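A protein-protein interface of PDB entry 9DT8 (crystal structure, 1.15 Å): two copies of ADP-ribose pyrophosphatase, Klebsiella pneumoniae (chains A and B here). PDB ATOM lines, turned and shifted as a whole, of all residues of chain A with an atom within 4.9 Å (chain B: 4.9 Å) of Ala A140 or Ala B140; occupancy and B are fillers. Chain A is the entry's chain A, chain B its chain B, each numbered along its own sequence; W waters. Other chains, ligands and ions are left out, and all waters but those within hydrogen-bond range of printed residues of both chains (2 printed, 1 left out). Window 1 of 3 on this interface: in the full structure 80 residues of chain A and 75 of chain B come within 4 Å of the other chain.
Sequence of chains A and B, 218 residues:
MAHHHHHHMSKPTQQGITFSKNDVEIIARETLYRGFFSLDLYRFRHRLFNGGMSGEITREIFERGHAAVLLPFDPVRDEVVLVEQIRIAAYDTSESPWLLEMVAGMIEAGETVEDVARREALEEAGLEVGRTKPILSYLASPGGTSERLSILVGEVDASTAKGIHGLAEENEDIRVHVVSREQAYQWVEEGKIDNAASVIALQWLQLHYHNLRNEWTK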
ATOM      1  N   TYR A 138      -6.216  26.469   1.897  1.00  0.00           N
ATOM      2  CA  TYR A 138      -6.627  26.406   3.294  1.00  0.00           C
ATOM      3  C   TYR A 138      -5.436  26.255   4.228  1.00  0.00           C
ATOM      4  O   TYR A 138      -4.384  25.751   3.847  1.00  0.00           O
ATOM      5  CB  TYR A 138      -7.635  25.251   3.549  1.00  0.00           C
ATOM      6  CG  TYR A 138      -7.004  23.869   3.432  1.00  0.00           C
ATOM      7  CD1 TYR A 138      -6.855  23.260   2.193  1.00  0.00           C
ATOM      8  CD2 TYR A 138      -6.552  23.183   4.558  1.00  0.00           C
ATOM      9  CE1 TYR A 138      -6.261  22.034   2.083  1.00  0.00           C
ATOM     10  CE2 TYR A 138      -5.959  21.942   4.447  1.00  0.00           C
ATOM     11  CZ  TYR A 138      -5.805  21.383   3.206  1.00  0.00           C
ATOM     12  OH  TYR A 138      -5.194  20.156   3.068  1.00  0.00           O
ATOM     13  N   LEU A 139      -5.620  26.717   5.457  1.00  0.00           N
ATOM     14  CA  LEU A 139      -4.703  26.510   6.567  1.00  0.00           C
ATOM     15  C   LEU A 139      -5.045  25.184   7.235  1.00  0.00           C
ATOM     16  O   LEU A 139      -6.183  24.977   7.681  1.00  0.00           O
ATOM     17  CB  LEU A 139      -4.864  27.672   7.540  1.00  0.00           C
ATOM     18  CG  LEU A 139      -4.416  29.036   7.006  1.00  0.00           C
ATOM     19  CD1 LEU A 139      -5.060  30.160   7.778  1.00  0.00           C
ATOM     20  CD2 LEU A 139      -2.882  29.159   7.061  1.00  0.00           C
ATOM     21  N   ALA A 140      -4.058  24.280   7.305  1.00  0.00           N
ATOM     22  CA  ALA A 140      -4.313  22.942   7.824  1.00  0.00           C
ATOM     23  C   ALA A 140      -4.760  22.932   9.276  1.00  0.00           C
ATOM     24  O   ALA A 140      -5.662  22.177   9.630  1.00  0.00           O
ATOM     25  CB  ALA A 140      -3.068  22.063   7.663  1.00  0.00           C
ATOM     26  N   SER A 141      -4.128  23.734  10.131  1.00  0.00           N
ATOM     27  CA  SER A 141      -4.412  23.722  11.566  1.00  0.00           C
ATOM     28  C   SER A 141      -3.778  24.952  12.192  1.00  0.00           C
ATOM     29  O   SER A 141      -2.712  24.868  12.818  1.00  0.00           O
ATOM     30  CB  SER A 141      -3.940  22.437  12.219  1.00  0.00           C
ATOM     31  OG  SER A 141      -4.341  22.450  13.573  1.00  0.00           O
ATOM     32  N   PRO A 142      -4.376  26.128  12.010  1.00  0.00           N
ATOM     33  CA  PRO A 142      -3.648  27.373  12.267  1.00  0.00           C
ATOM     34  C   PRO A 142      -3.467  27.733  13.730  1.00  0.00           C
ATOM     35  O   PRO A 142      -2.790  28.718  14.003  1.00  0.00           O
ATOM     36  CB  PRO A 142      -4.478  28.419  11.507  1.00  0.00           C
ATOM     37  CG  PRO A 142      -5.865  27.858  11.507  1.00  0.00           C
ATOM     38  CD  PRO A 142      -5.654  26.373  11.307  1.00  0.00           C
ATOM     39  N   THR A 145       0.235  25.341  13.458  1.00  0.00           N
ATOM     40  CA  THR A 145       1.101  25.224  12.295  1.00  0.00           C
ATOM     41  C   THR A 145       0.753  26.325  11.311  1.00  0.00           C
ATOM     42  O   THR A 145      -0.416  26.681  11.156  1.00  0.00           O
ATOM     43  CB  THR A 145       1.049  23.819  11.632  1.00  0.00           C
ATOM     44  OG1 THR A 145       1.972  23.788  10.542  1.00  0.00           O
ATOM     45  CG2 THR A 145      -0.313  23.460  11.090  1.00  0.00           C
ATOM     46  N   GLU A 147       1.103  25.948   8.135  1.00  0.00           N
ATOM     47  CA  GLU A 147       0.996  25.340   6.813  1.00  0.00           C
ATOM     48  C   GLU A 147      -0.287  25.746   6.100  1.00  0.00           C
ATOM     49  O   GLU A 147      -1.392  25.562   6.609  1.00  0.00           O
ATOM     50  CB  GLU A 147       1.053  23.823   6.926  1.00  0.00           C
ATOM     51  CG  GLU A 147       1.098  23.160   5.576  1.00  0.00           C
ATOM     52  CD  GLU A 147       1.065  21.642   5.615  1.00  0.00           C
ATOM     53  OE1 GLU A 147       0.513  21.062   6.572  1.00  0.00           O
ATOM     54  OE2 GLU A 147       1.540  21.044   4.628  1.00  0.00           O
ATOM     55  N   LEU A 149      -2.142  24.902   2.314  1.00  0.00           N
ATOM     56  CA  LEU A 149      -2.182  24.011   1.168  1.00  0.00           C
ATOM     57  C   LEU A 149      -3.166  24.562   0.150  1.00  0.00           C
ATOM     58  O   LEU A 149      -4.295  24.904   0.506  1.00  0.00           O
ATOM     59  CB  LEU A 149      -2.609  22.601   1.584  1.00  0.00           C
ATOM     60  CG  LEU A 149      -1.682  21.928   2.599  1.00  0.00           C
ATOM     61  CD1 LEU A 149      -2.169  22.140   4.029  1.00  0.00           C
ATOM     62  CD2 LEU A 149      -1.560  20.448   2.330  1.00  0.00           C
ATOM     63  N   ALA A 196      -7.290  15.873   5.637  1.00  0.00           N
ATOM     64  CA  ALA A 196      -7.945  17.131   5.277  1.00  0.00           C
ATOM     65  C   ALA A 196      -7.928  17.403   3.782  1.00  0.00           C
ATOM     66  O   ALA A 196      -8.952  17.777   3.210  1.00  0.00           O
ATOM     67  CB  ALA A 196      -7.307  18.301   6.023  1.00  0.00           C
ATOM     68  N   TYR B 138     -10.892  13.975  10.992  1.00  0.00           N
ATOM     69  CA  TYR B 138      -9.851  14.062   9.979  1.00  0.00           C
ATOM     70  C   TYR B 138      -8.484  14.336  10.575  1.00  0.00           C
ATOM     71  O   TYR B 138      -8.352  14.921  11.651  1.00  0.00           O
ATOM     72  CB  TYR B 138     -10.208  15.150   8.916  1.00  0.00           C
ATOM     73  CG  TYR B 138     -10.127  16.574   9.452  1.00  0.00           C
ATOM     74  CD1 TYR B 138     -11.194  17.148  10.140  1.00  0.00           C
ATOM     75  CD2 TYR B 138      -8.986  17.333   9.279  1.00  0.00           C
ATOM     76  CE1 TYR B 138     -11.121  18.444  10.635  1.00  0.00           C
ATOM     77  CE2 TYR B 138      -8.908  18.624   9.767  1.00  0.00           C
ATOM     78  CZ  TYR B 138      -9.963  19.160  10.473  1.00  0.00           C
ATOM     79  OH  TYR B 138      -9.892  20.425  10.991  1.00  0.00           O
ATOM     80  N   LEU B 139      -7.467  13.908   9.841  1.00  0.00           N
ATOM     81  CA  LEU B 139      -6.070  14.234  10.110  1.00  0.00           C
ATOM     82  C   LEU B 139      -5.752  15.557   9.415  1.00  0.00           C
ATOM     83  O   LEU B 139      -5.910  15.683   8.186  1.00  0.00           O
ATOM     84  CB  LEU B 139      -5.215  13.098   9.574  1.00  0.00           C
ATOM     85  CG  LEU B 139      -5.401  11.758  10.302  1.00  0.00           C
ATOM     86  CD1 LEU B 139      -4.901  10.601   9.434  1.00  0.00           C
ATOM     87  CD2 LEU B 139      -4.636  11.780  11.611  1.00  0.00           C
ATOM     88  N   ALA B 140      -5.287  16.531  10.193  1.00  0.00           N
ATOM     89  CA  ALA B 140      -5.045  17.865   9.652  1.00  0.00           C
ATOM     90  C   ALA B 140      -3.999  17.877   8.551  1.00  0.00           C
ATOM     91  O   ALA B 140      -4.171  18.592   7.557  1.00  0.00           O
ATOM     92  CB  ALA B 140      -4.642  18.819  10.772  1.00  0.00           C
ATOM     93  N   SER B 141      -2.900  17.170   8.727  1.00  0.00           N
ATOM     94  CA  SER B 141      -1.806  17.196   7.767  1.00  0.00           C
ATOM     95  C   SER B 141      -0.863  16.048   8.084  1.00  0.00           C
ATOM     96  O   SER B 141       0.208  16.247   8.684  1.00  0.00           O
ATOM     97  CB  SER B 141      -1.073  18.528   7.811  1.00  0.00           C
ATOM     98  OG  SER B 141      -0.102  18.559   6.795  1.00  0.00           O
ATOM     99  N   PRO B 142      -1.251  14.823   7.728  1.00  0.00           N
ATOM    100  CA  PRO B 142      -0.583  13.651   8.300  1.00  0.00           C
ATOM    101  C   PRO B 142       0.813  13.384   7.775  1.00  0.00           C
ATOM    102  O   PRO B 142       1.449  12.467   8.283  1.00  0.00           O
ATOM    103  CB  PRO B 142      -1.557  12.507   7.979  1.00  0.00           C
ATOM    104  CG  PRO B 142      -2.288  12.975   6.748  1.00  0.00           C
ATOM    105  CD  PRO B 142      -2.451  14.462   6.948  1.00  0.00           C
ATOM    106  N   THR B 145       2.177  15.964  11.030  1.00  0.00           N
ATOM    107  CA  THR B 145       1.596  16.071  12.364  1.00  0.00           C
ATOM    108  C   THR B 145       0.622  14.921  12.566  1.00  0.00           C
ATOM    109  O   THR B 145      -0.048  14.499  11.628  1.00  0.00           O
ATOM    110  CB  THR B 145       0.932  17.459  12.571  1.00  0.00           C
ATOM    111  OG1 THR B 145       0.387  17.520  13.893  1.00  0.00           O
ATOM    112  CG2 THR B 145      -0.205  17.727  11.591  1.00  0.00           C
ATOM    113  N   GLU B 147      -2.000  15.259  14.395  1.00  0.00           N
ATOM    114  CA  GLU B 147      -3.241  15.819  14.916  1.00  0.00           C
ATOM    115  C   GLU B 147      -4.465  15.328  14.163  1.00  0.00           C
ATOM    116  O   GLU B 147      -4.560  15.468  12.948  1.00  0.00           O
ATOM    117  CB  GLU B 147      -3.209  17.339  14.840  1.00  0.00           C
ATOM    118  CG  GLU B 147      -4.403  17.978  15.515  1.00  0.00           C
ATOM    119  CD  GLU B 147      -4.507  19.476  15.325  1.00  0.00           C
ATOM    120  OE1 GLU B 147      -3.936  20.010  14.342  1.00  0.00           O
ATOM    121  OE2 GLU B 147      -5.200  20.111  16.146  1.00  0.00           O
ATOM    122  N   LEU B 149      -8.723  15.904  14.298  1.00  0.00           N
ATOM    123  CA  LEU B 149      -9.799  16.765  14.751  1.00  0.00           C
ATOM    124  C   LEU B 149     -11.124  16.089  14.428  1.00  0.00           C
ATOM    125  O   LEU B 149     -11.370  15.697  13.275  1.00  0.00           O
ATOM    126  CB  LEU B 149      -9.724  18.150  14.087  1.00  0.00           C
ATOM    127  CG  LEU B 149      -8.452  18.949  14.359  1.00  0.00           C
ATOM    128  CD1 LEU B 149      -7.420  18.687  13.270  1.00  0.00           C
ATOM    129  CD2 LEU B 149      -8.663  20.421  14.488  1.00  0.00           C
ATOM    130  N   ALA B 196      -9.045  24.496   7.650  1.00  0.00           N
ATOM    131  CA  ALA B 196      -9.576  23.177   7.318  1.00  0.00           C
ATOM    132  C   ALA B 196     -10.848  22.849   8.087  1.00  0.00           C
ATOM    133  O   ALA B 196     -11.813  22.354   7.497  1.00  0.00           O
ATOM    134  CB  ALA B 196      -8.506  22.111   7.556  1.00  0.00           C
HETATM  135  O   HOH W   1      -3.842  18.776   4.904  1.00  0.00           O
HETATM  136  O   HOH W   2       1.572  18.514   3.748  1.00  0.00           O
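Of the 9 printed residues of chain A, 6 touch a printed residue of chain B. Hydrophobic or aromatic side chains of chain A that line the printed part of chain B: Tyr A138, Ala A140 and Ala A196. Among the printed residues, 10 pairs touch across the chains. Among the printed residues, no Asp or Glu carboxylate lies within 4 Å of a Lys or Arg side-chain nitrogen of the other chain.
The backbone carbonyl oxygen (O) of Leu A139 sits at hydrogen-bond distance from the backbone NH (N) of Ala B196 (2.9 Å). The side-chain hydroxyl of Ser A141 sits at hydrogen-bond distance from the side-chain carboxylate of Glu B147, at 2.6 Å. The side-chain carboxylate (OE1) of Glu A147 is in hydrogen-bond range of the side-chain hydroxyl (OG) of Ser B141 (2.6 Å). N of Ala A196 lies within hydrogen-bond range of O of Leu B139.
Ala A140 touches just these residues of chain B: Ala B140 and Ala B196. Thr A145 touches none of the printed residues of chain B. Printed residues of chain B within 4 Å of Glu A147: Ser B141 (2.6 Å). Of the printed residues of chain A, Tyr B138 touches Ala A196. Printed residues of chain A within 4 Å of Leu B139: Ala A196 (2.9 Å). Ala B140 touches just these residues of chain A: Ala A140, Ser A141 and Ala A196. Pro B142 touches none of the printed residues of chain A. The nearest printed residue of chain A that does not touch Ala B140 is Tyr A138 (4.9 Å).
Water W1 bridges OH of Tyr A138 (2.7 Å) and O of Ala B140 (2.7 Å). Water W2 bridges OE2 of Glu A147 (2.7 Å) and OG of Ser B141 (3.5 Å).
Leu A139 touches Ala B196, and with the chains exchanged Ala A196 touches Leu B139. Ala B140 touches its own counterpart, Ala A140. Ala A140 touches Ala B196, and with the chains exchanged Ala A196 touches Ala B140. Ser A141 touches Glu B147, and with the chains exchanged Glu A147 touches Ser B141. 9 positions are printed for both chains. Of the 10 pairs that touch across the chains among the printed residues, 9 have their exchanged pair printed and touching as well.
The backbone NH (N) of Tyr A138 is in hydrogen-bond range of the backbone carbonyl oxygen (O) of Leu A149 (2.8 Å). N of Ala A140 lies within hydrogen-bond range of O of Glu A147, at 3.0 Å. N of Glu A147 lies close to OG1 of Thr A145 (3.3 Å). O of Tyr B138 is in hydrogen-bond range of N of Leu B149, 2.8 Å away. The backbone carbonyl oxygen (O) of Glu B147 lies within hydrogen-bond range of the backbone NH (N) of Ala B140, at 3.0 Å. The side-chain hydroxyl (OG1) of Thr B145 lies close to the backbone NH (N) of Glu B147, 3.3 Å away.
Tyr A138 touches Ala B196. O of Ala B140 touches CB of Ala A140 (3.6 Å). Ala A140 touches Ala B196 (O to CB, 3.5 Å). Ser A141 touches Ala B140. Tyr B138 touches Ala A196. Ala A196 touches Ala B140 (CB to O, 3.5 Å).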
